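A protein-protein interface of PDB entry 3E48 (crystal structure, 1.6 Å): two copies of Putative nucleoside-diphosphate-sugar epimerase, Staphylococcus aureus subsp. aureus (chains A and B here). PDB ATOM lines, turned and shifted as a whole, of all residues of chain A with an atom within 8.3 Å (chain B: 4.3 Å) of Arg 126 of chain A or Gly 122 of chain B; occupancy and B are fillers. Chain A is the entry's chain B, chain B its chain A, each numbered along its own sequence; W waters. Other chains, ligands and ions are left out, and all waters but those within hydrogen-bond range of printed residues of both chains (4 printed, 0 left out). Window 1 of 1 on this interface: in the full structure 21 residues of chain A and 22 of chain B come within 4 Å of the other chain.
Among the printed residues, merely in contact across the chains: Ser 118 of chain A with Arg 126 of chain B, Arg 126 of chain A with Ser 118 of chain B, Arg 194 of chain A with His 111 of chain B, Tyr 123 of chain A with Pro 119 of chain B, Pro 119 of chain A with Tyr 123 of chain B, Leu 127 of chain A with Pro 119 of chain B, Arg 126 of chain A with Gly 122 of chain B, Gly 122 of chain A with Arg 126 of chain B, Arg 126 of chain A with Pro 119 of chain B, Thr 130 of chain A with Ser 118 of chain B, Pro 119 of chain A with Arg 126 of chain B, Thr 130 of chain A with Pro 119 of chain B and Tyr 123 of chain A with Tyr 123 of chain B.
His 111 of chain A touches Arg 126 of chain B, and with the chains exchanged Arg 126 of chain A touches His 111 of chain B.
Ser 118 of chain A touches Arg 126 of chain B, and with the chains exchanged Arg 126 of chain A touches Ser 118 of chain B.
Tyr 123 of chain A touches its own counterpart, Tyr 123 of chain B.
The guanidinium group of Arg 126 of chain B sits at hydrogen-bond distance from the backbone carbonyl oxygen of Gln 110 of chain A, at 3.4 Å.
The side-chain hydroxyl (OG) of Ser 125 of chain A is in hydrogen-bond range of the backbone carbonyl oxygen (O) of His 111 of chain B (3.0 Å).
The backbone carbonyl oxygen (O) of His 111 of chain A is in hydrogen-bond range of the side-chain hydroxyl (OG) of Ser 125 of chain B (3.2 Å).
O of Gln 110 of chain B is in hydrogen-bond range of NE of Arg 126 of chain A.
The guanidinium group of Arg 126 of chain B is in hydrogen-bond range of the backbone carbonyl oxygen of Asp 109 of chain A.
O of Asp 109 of chain B lies within hydrogen-bond range of NE of Arg 126 of chain A (2.8 Å).
The guanidinium group of Arg 126 of chain B sits close to the guanidinium group of Arg 126 of chain A (3.3 Å).
The backbone NH of His 111 of chain A sits close to the guanidinium group of Arg 126 of chain B (3.2 Å).
NH2 of Arg 126 of chain A lies close to N of His 111 of chain B (3.3 Å).
The side-chain hydroxyl of Ser 125 of chain A is in hydrogen-bond range of the guanidinium group of Arg 194 of chain A, 3.1 Å away.
The guanidinium group of Arg 126 of chain B sits at hydrogen-bond distance from the backbone carbonyl oxygen of Gly 122 of chain B (2.9 Å).
Of the 24 printed residues of chain A, 12 touch a printed residue of chain B.
Hydrophobic or aromatic side chains of chain B within 4 Å of the printed part of chain A: His 111, Pro 119 and Tyr 123.
Among the printed residues, no Asp or Glu carboxylate lies within 4 Å of a Lys or Arg side-chain nitrogen of the other chain.
Of the printed residues of chain B, Gln 110 of chain A touches Arg 126 (3.4 Å).
Of chain B, only Asp 109, Gln 110, His 111, Ser 118, Pro 119, Gly 122 and Arg 126 come within 4 Å of Arg 126 of chain A.
Gly 132 of chain A touches none of the printed residues of chain B.
Of the printed residues of chain A, Gln 110 of chain B touches Arg 126 (3.4 Å).
Of chain A, only Tyr 123 (3.5 Å), Arg 126 (3.7 Å), Leu 127 (3.5 Å) and Thr 130 (3.8 Å) come within 4 Å of Pro 119 of chain B.
Tyr 120 of chain B touches none of the printed residues of chain A.
Gly 122 of chain B touches one residue of chain A.
Water W4 lies within hydrogen-bond range of OH of Tyr 135 of chain A (2.6 Å), O of His 111 of chain B (2.7 Å), OG of Ser 125 of chain A (2.9 Å) and NH2 of Arg 194 of chain A (3.2 Å).
Water W2 lies within hydrogen-bond range of NH1 of Arg 126 of chain A and NH2 of Arg 126 of chain B.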
ATOM      1  N   VAL A  86       9.469  29.044 -34.145  1.00  0.00           N
ATOM      2  CA  VAL A  86       8.442  29.849 -33.495  1.00  0.00           C
ATOM      3  C   VAL A  86       9.058  31.028 -32.760  1.00  0.00           C
ATOM      4  O   VAL A  86       8.446  32.085 -32.669  1.00  0.00           O
ATOM      5  CB  VAL A  86       7.597  29.002 -32.503  1.00  0.00           C
ATOM      6  CG1 VAL A  86       8.466  28.482 -31.370  1.00  0.00           C
ATOM      7  CG2 VAL A  86       6.444  29.838 -31.962  1.00  0.00           C
ATOM      8  N   VAL A  90       7.774  34.922 -33.566  1.00  0.00           N
ATOM      9  CA  VAL A  90       7.383  35.936 -32.589  1.00  0.00           C
ATOM     10  C   VAL A  90       8.320  37.143 -32.583  1.00  0.00           C
ATOM     11  O   VAL A  90       7.864  38.286 -32.542  1.00  0.00           O
ATOM     12  CB  VAL A  90       7.314  35.345 -31.161  1.00  0.00           C
ATOM     13  CG1 VAL A  90       7.027  36.449 -30.152  1.00  0.00           C
ATOM     14  CG2 VAL A  90       6.228  34.279 -31.097  1.00  0.00           C
ATOM     15  N   ASP A 109      -1.188  17.413 -29.834  1.00  0.00           N
ATOM     16  CA  ASP A 109      -0.486  18.330 -28.949  1.00  0.00           C
ATOM     17  C   ASP A 109      -0.887  18.350 -27.472  1.00  0.00           C
ATOM     18  O   ASP A 109      -0.566  19.307 -26.767  1.00  0.00           O
ATOM     19  CB  ASP A 109      -0.623  19.749 -29.514  1.00  0.00           C
ATOM     20  CG  ASP A 109      -2.063  20.242 -29.522  1.00  0.00           C
ATOM     21  OD1 ASP A 109      -2.976  19.489 -29.110  1.00  0.00           O
ATOM     22  OD2 ASP A 109      -2.293  21.398 -29.950  1.00  0.00           O
ATOM     23  N   GLN A 110      -1.576  17.317 -26.994  1.00  0.00           N
ATOM     24  CA  GLN A 110      -1.978  17.295 -25.588  1.00  0.00           C
ATOM     25  C   GLN A 110      -0.766  17.111 -24.682  1.00  0.00           C
ATOM     26  O   GLN A 110       0.286  16.652 -25.126  1.00  0.00           O
ATOM     27  CB  GLN A 110      -2.998  16.183 -25.328  1.00  0.00           C
ATOM     28  CG  GLN A 110      -4.262  16.304 -26.180  1.00  0.00           C
ATOM     29  CD  GLN A 110      -4.249  15.364 -27.373  1.00  0.00           C
ATOM     30  OE1 GLN A 110      -3.220  15.194 -28.033  1.00  0.00           O
ATOM     31  NE2 GLN A 110      -5.400  14.755 -27.665  1.00  0.00           N
ATOM     32  N   HIS A 111      -0.916  17.460 -23.408  1.00  0.00           N
ATOM     33  CA  HIS A 111       0.191  17.347 -22.461  1.00  0.00           C
ATOM     34  C   HIS A 111       0.753  15.934 -22.359  1.00  0.00           C
ATOM     35  O   HIS A 111       1.924  15.751 -22.012  1.00  0.00           O
ATOM     36  CB  HIS A 111      -0.246  17.813 -21.067  1.00  0.00           C
ATOM     37  CG  HIS A 111      -1.251  16.914 -20.417  1.00  0.00           C
ATOM     38  ND1 HIS A 111      -2.605  17.019 -20.644  1.00  0.00           N
ATOM     39  CD2 HIS A 111      -1.093  15.883 -19.553  1.00  0.00           C
ATOM     40  CE1 HIS A 111      -3.240  16.094 -19.947  1.00  0.00           C
ATOM     41  NE2 HIS A 111      -2.347  15.390 -19.277  1.00  0.00           N
ATOM     42  N   ASN A 112      -0.081  14.940 -22.654  1.00  0.00           N
ATOM     43  CA  ASN A 112       0.343  13.543 -22.584  1.00  0.00           C
ATOM     44  C   ASN A 112       0.361  12.848 -23.946  1.00  0.00           C
ATOM     45  O   ASN A 112       0.239  11.626 -24.032  1.00  0.00           O
ATOM     46  CB  ASN A 112      -0.559  12.767 -21.612  1.00  0.00           C
ATOM     47  CG  ASN A 112      -2.004  12.693 -22.077  1.00  0.00           C
ATOM     48  OD1 ASN A 112      -2.467  13.528 -22.852  1.00  0.00           O
ATOM     49  ND2 ASN A 112      -2.731  11.694 -21.586  1.00  0.00           N
ATOM     50  N   SER A 118       4.901  16.683 -30.336  1.00  0.00           N
ATOM     51  CA  SER A 118       3.971  17.353 -29.429  1.00  0.00           C
ATOM     52  C   SER A 118       4.641  18.484 -28.627  1.00  0.00           C
ATOM     53  O   SER A 118       4.030  19.528 -28.410  1.00  0.00           O
ATOM     54  CB  SER A 118       3.290  16.348 -28.479  1.00  0.00           C
ATOM     55  OG  SER A 118       4.183  15.830 -27.525  1.00  0.00           O
ATOM     56  N   PRO A 119       5.906  18.304 -28.197  1.00  0.00           N
ATOM     57  CA  PRO A 119       6.549  19.382 -27.435  1.00  0.00           C
ATOM     58  C   PRO A 119       6.584  20.691 -28.230  1.00  0.00           C
ATOM     59  O   PRO A 119       6.351  21.771 -27.681  1.00  0.00           O
ATOM     60  CB  PRO A 119       7.951  18.834 -27.169  1.00  0.00           C
ATOM     61  CG  PRO A 119       7.733  17.354 -27.119  1.00  0.00           C
ATOM     62  CD  PRO A 119       6.800  17.134 -28.293  1.00  0.00           C
ATOM     63  N   TYR A 120       6.878  20.587 -29.524  1.00  0.00           N
ATOM     64  CA  TYR A 120       6.934  21.771 -30.378  1.00  0.00           C
ATOM     65  C   TYR A 120       5.598  22.492 -30.429  1.00  0.00           C
ATOM     66  O   TYR A 120       5.542  23.709 -30.265  1.00  0.00           O
ATOM     67  CB  TYR A 120       7.345  21.400 -31.806  1.00  0.00           C
ATOM     68  CG  TYR A 120       7.157  22.532 -32.800  1.00  0.00           C
ATOM     69  CD1 TYR A 120       8.082  23.576 -32.885  1.00  0.00           C
ATOM     70  CD2 TYR A 120       6.037  22.577 -33.636  1.00  0.00           C
ATOM     71  CE1 TYR A 120       7.901  24.633 -33.778  1.00  0.00           C
ATOM     72  CE2 TYR A 120       5.845  23.634 -34.531  1.00  0.00           C
ATOM     73  CZ  TYR A 120       6.781  24.654 -34.596  1.00  0.00           C
ATOM     74  OH  TYR A 120       6.611  25.698 -35.487  1.00  0.00           O
ATOM     75  N   PHE A 121       4.521  21.749 -30.649  1.00  0.00           N
ATOM     76  CA  PHE A 121       3.208  22.374 -30.744  1.00  0.00           C
ATOM     77  C   PHE A 121       2.720  22.922 -29.415  1.00  0.00           C
ATOM     78  O   PHE A 121       2.067  23.965 -29.372  1.00  0.00           O
ATOM     79  CB  PHE A 121       2.212  21.393 -31.357  1.00  0.00           C
ATOM     80  CG  PHE A 121       2.473  21.130 -32.811  1.00  0.00           C
ATOM     81  CD1 PHE A 121       2.277  22.141 -33.751  1.00  0.00           C
ATOM     82  CD2 PHE A 121       2.971  19.906 -33.235  1.00  0.00           C
ATOM     83  CE1 PHE A 121       2.580  21.940 -35.098  1.00  0.00           C
ATOM     84  CE2 PHE A 121       3.280  19.687 -34.581  1.00  0.00           C
ATOM     85  CZ  PHE A 121       3.083  20.708 -35.514  1.00  0.00           C
ATOM     86  N   GLY A 122       3.036  22.232 -28.324  1.00  0.00           N
ATOM     87  CA  GLY A 122       2.637  22.742 -27.028  1.00  0.00           C
ATOM     88  C   GLY A 122       3.386  24.038 -26.768  1.00  0.00           C
ATOM     89  O   GLY A 122       2.819  25.011 -26.277  1.00  0.00           O
ATOM     90  N   TYR A 123       4.673  24.047 -27.102  1.00  0.00           N
ATOM     91  CA  TYR A 123       5.514  25.218 -26.908  1.00  0.00           C
ATOM     92  C   TYR A 123       5.059  26.401 -27.755  1.00  0.00           C
ATOM     93  O   TYR A 123       4.997  27.531 -27.268  1.00  0.00           O
ATOM     94  CB  TYR A 123       6.960  24.853 -27.241  1.00  0.00           C
ATOM     95  CG  TYR A 123       7.987  25.922 -26.950  1.00  0.00           C
ATOM     96  CD1 TYR A 123       8.220  26.966 -27.851  1.00  0.00           C
ATOM     97  CD2 TYR A 123       8.775  25.852 -25.799  1.00  0.00           C
ATOM     98  CE1 TYR A 123       9.225  27.910 -27.615  1.00  0.00           C
ATOM     99  CE2 TYR A 123       9.774  26.786 -25.554  1.00  0.00           C
ATOM    100  CZ  TYR A 123       9.998  27.808 -26.464  1.00  0.00           C
ATOM    101  OH  TYR A 123      11.015  28.702 -26.223  1.00  0.00           O
ATOM    102  N   ALA A 124       4.741  26.133 -29.019  1.00  0.00           N
ATOM    103  CA  ALA A 124       4.298  27.169 -29.951  1.00  0.00           C
ATOM    104  C   ALA A 124       3.048  27.901 -29.462  1.00  0.00           C
ATOM    105  O   ALA A 124       3.008  29.137 -29.435  1.00  0.00           O
ATOM    106  CB  ALA A 124       4.039  26.550 -31.324  1.00  0.00           C
ATOM    107  N   SER A 125       2.027  27.138 -29.085  1.00  0.00           N
ATOM    108  CA  SER A 125       0.776  27.716 -28.603  1.00  0.00           C
ATOM    109  C   SER A 125       1.039  28.639 -27.417  1.00  0.00           C
ATOM    110  O   SER A 125       0.580  29.785 -27.380  1.00  0.00           O
ATOM    111  CB  SER A 125      -0.194  26.598 -28.197  1.00  0.00           C
ATOM    112  OG  SER A 125      -1.417  27.121 -27.713  1.00  0.00           O
ATOM    113  N   ARG A 126       1.790  28.139 -26.445  1.00  0.00           N
ATOM    114  CA  ARG A 126       2.100  28.932 -25.261  1.00  0.00           C
ATOM    115  C   ARG A 126       2.965  30.153 -25.574  1.00  0.00           C
ATOM    116  O   ARG A 126       2.723  31.237 -25.039  1.00  0.00           O
ATOM    117  CB  ARG A 126       2.761  28.030 -24.215  1.00  0.00           C
ATOM    118  CG  ARG A 126       1.798  26.942 -23.768  1.00  0.00           C
ATOM    119  CD  ARG A 126       2.457  25.794 -23.025  1.00  0.00           C
ATOM    120  NE  ARG A 126       1.429  24.918 -22.463  1.00  0.00           N
ATOM    121  CZ  ARG A 126       0.643  24.116 -23.178  1.00  0.00           C
ATOM    122  NH1 ARG A 126       0.762  24.054 -24.501  1.00  0.00           N
ATOM    123  NH2 ARG A 126      -0.296  23.398 -22.570  1.00  0.00           N
ATOM    124  N   LEU A 127       3.955  29.999 -26.450  1.00  0.00           N
ATOM    125  CA  LEU A 127       4.803  31.138 -26.786  1.00  0.00           C
ATOM    126  C   LEU A 127       3.950  32.248 -27.399  1.00  0.00           C
ATOM    127  O   LEU A 127       4.149  33.428 -27.107  1.00  0.00           O
ATOM    128  CB  LEU A 127       5.911  30.743 -27.766  1.00  0.00           C
ATOM    129  CG  LEU A 127       7.020  31.793 -27.957  1.00  0.00           C
ATOM    130  CD1 LEU A 127       7.812  31.958 -26.650  1.00  0.00           C
ATOM    131  CD2 LEU A 127       7.940  31.367 -29.086  1.00  0.00           C
ATOM    132  N   LEU A 128       3.000  31.879 -28.254  1.00  0.00           N
ATOM    133  CA  LEU A 128       2.135  32.890 -28.856  1.00  0.00           C
ATOM    134  C   LEU A 128       1.357  33.599 -27.754  1.00  0.00           C
ATOM    135  O   LEU A 128       1.207  34.819 -27.773  1.00  0.00           O
ATOM    136  CB  LEU A 128       1.178  32.248 -29.866  1.00  0.00           C
ATOM    137  CG  LEU A 128       1.892  31.868 -31.165  1.00  0.00           C
ATOM    138  CD1 LEU A 128       1.052  30.875 -31.951  1.00  0.00           C
ATOM    139  CD2 LEU A 128       2.151  33.125 -31.989  1.00  0.00           C
ATOM    140  N   SER A 129       0.870  32.828 -26.785  1.00  0.00           N
ATOM    141  CA  SER A 129       0.126  33.402 -25.672  1.00  0.00           C
ATOM    142  C   SER A 129       0.986  34.399 -24.882  1.00  0.00           C
ATOM    143  O   SER A 129       0.507  35.468 -24.505  1.00  0.00           O
ATOM    144  CB  SER A 129      -0.371  32.285 -24.744  1.00  0.00           C
ATOM    145  OG  SER A 129      -1.122  32.819 -23.666  1.00  0.00           O
ATOM    146  N   THR A 130       2.256  34.067 -24.649  1.00  0.00           N
ATOM    147  CA  THR A 130       3.135  34.959 -23.884  1.00  0.00           C
ATOM    148  C   THR A 130       3.601  36.194 -24.652  1.00  0.00           C
ATOM    149  O   THR A 130       4.000  37.188 -24.041  1.00  0.00           O
ATOM    150  CB  THR A 130       4.427  34.257 -23.412  1.00  0.00           C
ATOM    151  OG1 THR A 130       5.303  34.061 -24.532  1.00  0.00           O
ATOM    152  CG2 THR A 130       4.113  32.913 -22.771  1.00  0.00           C
ATOM    153  N   SER A 131       3.547  36.130 -25.980  1.00  0.00           N
ATOM    154  CA  SER A 131       4.012  37.223 -26.843  1.00  0.00           C
ATOM    155  C   SER A 131       3.231  38.530 -26.777  1.00  0.00           C
ATOM    156  O   SER A 131       3.795  39.601 -27.006  1.00  0.00           O
ATOM    157  CB  SER A 131       4.037  36.762 -28.299  1.00  0.00           C
ATOM    158  OG  SER A 131       2.721  36.658 -28.798  1.00  0.00           O
ATOM    159  N   GLY A 132       1.935  38.446 -26.498  1.00  0.00           N
ATOM    160  CA  GLY A 132       1.129  39.652 -26.445  1.00  0.00           C
ATOM    161  C   GLY A 132       0.630  40.064 -27.819  1.00  0.00           C
ATOM    162  O   GLY A 132      -0.065  41.070 -27.965  1.00  0.00           O
ATOM    163  N   TYR A 135      -3.426  36.582 -32.012  1.00  0.00           N
ATOM    164  CA  TYR A 135      -3.226  35.399 -32.832  1.00  0.00           C
ATOM    165  C   TYR A 135      -4.445  34.486 -32.880  1.00  0.00           C
ATOM    166  O   TYR A 135      -5.334  34.555 -32.030  1.00  0.00           O
ATOM    167  CB  TYR A 135      -1.997  34.598 -32.358  1.00  0.00           C
ATOM    168  CG  TYR A 135      -2.170  33.909 -31.021  1.00  0.00           C
ATOM    169  CD1 TYR A 135      -2.118  34.630 -29.827  1.00  0.00           C
ATOM    170  CD2 TYR A 135      -2.411  32.536 -30.953  1.00  0.00           C
ATOM    171  CE1 TYR A 135      -2.307  33.995 -28.596  1.00  0.00           C
ATOM    172  CE2 TYR A 135      -2.599  31.896 -29.734  1.00  0.00           C
ATOM    173  CZ  TYR A 135      -2.549  32.629 -28.563  1.00  0.00           C
ATOM    174  OH  TYR A 135      -2.761  31.992 -27.360  1.00  0.00           O
ATOM    175  N   TYR A 137      -5.102  30.406 -33.372  1.00  0.00           N
ATOM    176  CA  TYR A 137      -4.438  29.111 -33.402  1.00  0.00           C
ATOM    177  C   TYR A 137      -5.358  28.083 -34.056  1.00  0.00           C
ATOM    178  O   TYR A 137      -6.428  27.757 -33.537  1.00  0.00           O
ATOM    179  CB  TYR A 137      -4.054  28.698 -31.977  1.00  0.00           C
ATOM    180  CG  TYR A 137      -2.961  27.659 -31.928  1.00  0.00           C
ATOM    181  CD1 TYR A 137      -3.261  26.301 -31.995  1.00  0.00           C
ATOM    182  CD2 TYR A 137      -1.619  28.037 -31.880  1.00  0.00           C
ATOM    183  CE1 TYR A 137      -2.247  25.338 -32.023  1.00  0.00           C
ATOM    184  CE2 TYR A 137      -0.598  27.084 -31.909  1.00  0.00           C
ATOM    185  CZ  TYR A 137      -0.922  25.739 -31.982  1.00  0.00           C
ATOM    186  OH  TYR A 137       0.070  24.789 -32.023  1.00  0.00           O
ATOM    187  N   ARG A 194      -9.486  29.830 -31.054  1.00  0.00           N
ATOM    188  CA  ARG A 194      -8.775  28.574 -31.257  1.00  0.00           C
ATOM    189  C   ARG A 194      -9.703  27.668 -32.056  1.00  0.00           C
ATOM    190  O   ARG A 194     -10.866  27.495 -31.697  1.00  0.00           O
ATOM    191  CB  ARG A 194      -8.449  27.941 -29.900  1.00  0.00           C
ATOM    192  CG  ARG A 194      -7.382  26.859 -29.939  1.00  0.00           C
ATOM    193  CD  ARG A 194      -7.068  26.369 -28.522  1.00  0.00           C
ATOM    194  NE  ARG A 194      -5.968  25.407 -28.483  1.00  0.00           N
ATOM    195  CZ  ARG A 194      -4.680  25.730 -28.565  1.00  0.00           C
ATOM    196  NH1 ARG A 194      -3.757  24.781 -28.520  1.00  0.00           N
ATOM    197  NH2 ARG A 194      -4.309  26.999 -28.678  1.00  0.00           N
ATOM    198  N   ASP B 109       0.632  26.455 -16.832  1.00  0.00           N
ATOM    199  CA  ASP B 109       1.054  25.754 -18.036  1.00  0.00           C
ATOM    200  C   ASP B 109      -0.011  25.464 -19.092  1.00  0.00           C
ATOM    201  O   ASP B 109       0.210  24.618 -19.963  1.00  0.00           O
ATOM    202  CB  ASP B 109       1.707  24.426 -17.635  1.00  0.00           C
ATOM    203  CG  ASP B 109       0.755  23.509 -16.881  1.00  0.00           C
ATOM    204  OD1 ASP B 109      -0.436  23.864 -16.727  1.00  0.00           O
ATOM    205  OD2 ASP B 109       1.196  22.421 -16.440  1.00  0.00           O
ATOM    206  N   GLN B 110      -1.161  26.131 -19.028  1.00  0.00           N
ATOM    207  CA  GLN B 110      -2.205  25.885 -20.034  1.00  0.00           C
ATOM    208  C   GLN B 110      -1.773  26.395 -21.402  1.00  0.00           C
ATOM    209  O   GLN B 110      -0.888  27.248 -21.507  1.00  0.00           O
ATOM    210  CB  GLN B 110      -3.528  26.553 -19.643  1.00  0.00           C
ATOM    211  CG  GLN B 110      -4.087  26.057 -18.322  1.00  0.00           C
ATOM    212  CD  GLN B 110      -3.783  26.999 -17.182  1.00  0.00           C
ATOM    213  OE1 GLN B 110      -2.738  27.643 -17.159  1.00  0.00           O
ATOM    214  NE2 GLN B 110      -4.697  27.079 -16.222  1.00  0.00           N
ATOM    215  N   HIS B 111      -2.404  25.882 -22.453  1.00  0.00           N
ATOM    216  CA  HIS B 111      -2.051  26.292 -23.810  1.00  0.00           C
ATOM    217  C   HIS B 111      -2.195  27.789 -24.039  1.00  0.00           C
ATOM    218  O   HIS B 111      -1.564  28.347 -24.938  1.00  0.00           O
ATOM    219  CB  HIS B 111      -2.908  25.555 -24.843  1.00  0.00           C
ATOM    220  CG  HIS B 111      -4.367  25.884 -24.760  1.00  0.00           C
ATOM    221  ND1 HIS B 111      -5.217  25.277 -23.861  1.00  0.00           N
ATOM    222  CD2 HIS B 111      -5.119  26.778 -25.444  1.00  0.00           C
ATOM    223  CE1 HIS B 111      -6.430  25.783 -23.996  1.00  0.00           C
ATOM    224  NE2 HIS B 111      -6.397  26.696 -24.948  1.00  0.00           N
ATOM    225  N   SER B 118       5.341  29.519 -19.292  1.00  0.00           N
ATOM    226  CA  SER B 118       4.418  28.460 -19.679  1.00  0.00           C
ATOM    227  C   SER B 118       4.942  27.598 -20.837  1.00  0.00           C
ATOM    228  O   SER B 118       4.755  26.384 -20.829  1.00  0.00           O
ATOM    229  CB  SER B 118       3.017  29.017 -19.997  1.00  0.00           C
ATOM    230  OG  SER B 118       2.987  29.783 -21.181  1.00  0.00           O
ATOM    231  N   PRO B 119       5.627  28.198 -21.832  1.00  0.00           N
ATOM    232  CA  PRO B 119       6.119  27.340 -22.924  1.00  0.00           C
ATOM    233  C   PRO B 119       7.055  26.227 -22.416  1.00  0.00           C
ATOM    234  O   PRO B 119       7.004  25.093 -22.899  1.00  0.00           O
ATOM    235  CB  PRO B 119       6.835  28.323 -23.844  1.00  0.00           C
ATOM    236  CG  PRO B 119       6.053  29.597 -23.646  1.00  0.00           C
ATOM    237  CD  PRO B 119       5.850  29.624 -22.142  1.00  0.00           C
ATOM    238  N   TYR B 120       7.909  26.556 -21.448  1.00  0.00           N
ATOM    239  CA  TYR B 120       8.828  25.568 -20.887  1.00  0.00           C
ATOM    240  C   TYR B 120       8.075  24.423 -20.227  1.00  0.00           C
ATOM    241  O   TYR B 120       8.402  23.252 -20.431  1.00  0.00           O
ATOM    242  CB  TYR B 120       9.755  26.213 -19.847  1.00  0.00           C
ATOM    243  CG  TYR B 120      10.540  25.212 -19.011  1.00  0.00           C
ATOM    244  CD1 TYR B 120      11.726  24.649 -19.485  1.00  0.00           C
ATOM    245  CD2 TYR B 120      10.074  24.811 -17.752  1.00  0.00           C
ATOM    246  CE1 TYR B 120      12.431  23.711 -18.730  1.00  0.00           C
ATOM    247  CE2 TYR B 120      10.770  23.876 -16.986  1.00  0.00           C
ATOM    248  CZ  TYR B 120      11.948  23.330 -17.483  1.00  0.00           C
ATOM    249  OH  TYR B 120      12.647  22.403 -16.737  1.00  0.00           O
ATOM    250  N   PHE B 121       7.065  24.753 -19.432  1.00  0.00           N
ATOM    251  CA  PHE B 121       6.324  23.708 -18.743  1.00  0.00           C
ATOM    252  C   PHE B 121       5.464  22.871 -19.686  1.00  0.00           C
ATOM    253  O   PHE B 121       5.316  21.663 -19.482  1.00  0.00           O
ATOM    254  CB  PHE B 121       5.516  24.317 -17.595  1.00  0.00           C
ATOM    255  CG  PHE B 121       6.388  24.811 -16.463  1.00  0.00           C
ATOM    256  CD1 PHE B 121       7.091  23.904 -15.667  1.00  0.00           C
ATOM    257  CD2 PHE B 121       6.556  26.173 -16.236  1.00  0.00           C
ATOM    258  CE1 PHE B 121       7.954  24.347 -14.661  1.00  0.00           C
ATOM    259  CE2 PHE B 121       7.417  26.633 -15.232  1.00  0.00           C
ATOM    260  CZ  PHE B 121       8.118  25.721 -14.445  1.00  0.00           C
ATOM    261  N   GLY B 122       4.911  23.494 -20.724  1.00  0.00           N
ATOM    262  CA  GLY B 122       4.130  22.730 -21.679  1.00  0.00           C
ATOM    263  C   GLY B 122       5.067  21.790 -22.424  1.00  0.00           C
ATOM    264  O   GLY B 122       4.744  20.630 -22.676  1.00  0.00           O
ATOM    265  N   TYR B 123       6.246  22.295 -22.770  1.00  0.00           N
ATOM    266  CA  TYR B 123       7.233  21.505 -23.490  1.00  0.00           C
ATOM    267  C   TYR B 123       7.743  20.338 -22.642  1.00  0.00           C
ATOM    268  O   TYR B 123       7.848  19.215 -23.125  1.00  0.00           O
ATOM    269  CB  TYR B 123       8.392  22.418 -23.913  1.00  0.00           C
ATOM    270  CG  TYR B 123       9.464  21.785 -24.774  1.00  0.00           C
ATOM    271  CD1 TYR B 123      10.497  21.035 -24.207  1.00  0.00           C
ATOM    272  CD2 TYR B 123       9.490  22.001 -26.151  1.00  0.00           C
ATOM    273  CE1 TYR B 123      11.535  20.525 -24.992  1.00  0.00           C
ATOM    274  CE2 TYR B 123      10.519  21.500 -26.943  1.00  0.00           C
ATOM    275  CZ  TYR B 123      11.539  20.766 -26.360  1.00  0.00           C
ATOM    276  OH  TYR B 123      12.568  20.303 -27.152  1.00  0.00           O
ATOM    277  N   ALA B 124       8.038  20.600 -21.372  1.00  0.00           N
ATOM    278  CA  ALA B 124       8.558  19.561 -20.486  1.00  0.00           C
ATOM    279  C   ALA B 124       7.607  18.375 -20.341  1.00  0.00           C
ATOM    280  O   ALA B 124       8.019  17.223 -20.483  1.00  0.00           O
ATOM    281  CB  ALA B 124       8.870  20.156 -19.113  1.00  0.00           C
ATOM    282  N   SER B 125       6.343  18.659 -20.052  1.00  0.00           N
ATOM    283  CA  SER B 125       5.351  17.603 -19.886  1.00  0.00           C
ATOM    284  C   SER B 125       5.285  16.728 -21.137  1.00  0.00           C
ATOM    285  O   SER B 125       5.302  15.494 -21.058  1.00  0.00           O
ATOM    286  CB  SER B 125       3.977  18.217 -19.595  1.00  0.00           C
ATOM    287  OG  SER B 125       2.989  17.217 -19.433  1.00  0.00           O
ATOM    288  N   ARG B 126       5.224  17.373 -22.296  1.00  0.00           N
ATOM    289  CA  ARG B 126       5.154  16.655 -23.561  1.00  0.00           C
ATOM    290  C   ARG B 126       6.428  15.871 -23.872  1.00  0.00           C
ATOM    291  O   ARG B 126       6.358  14.721 -24.320  1.00  0.00           O
ATOM    292  CB  ARG B 126       4.809  17.650 -24.678  1.00  0.00           C
ATOM    293  CG  ARG B 126       3.400  18.215 -24.509  1.00  0.00           C
ATOM    294  CD  ARG B 126       3.095  19.438 -25.376  1.00  0.00           C
ATOM    295  NE  ARG B 126       1.685  19.795 -25.235  1.00  0.00           N
ATOM    296  CZ  ARG B 126       1.144  20.294 -24.128  1.00  0.00           C
ATOM    297  NH1 ARG B 126       1.897  20.521 -23.056  1.00  0.00           N
ATOM    298  NH2 ARG B 126      -0.162  20.516 -24.070  1.00  0.00           N
HETATM  299  O   HOH W   1       0.796  21.302 -20.477  1.00  0.00           O
HETATM  300  O   HOH W   2      -1.331  22.797 -26.174  1.00  0.00           O
HETATM  301  O   HOH W   3       2.407  14.628 -19.681  1.00  0.00           O
HETATM  302  O   HOH W   4      -3.029  29.396 -27.002  1.00  0.00           O
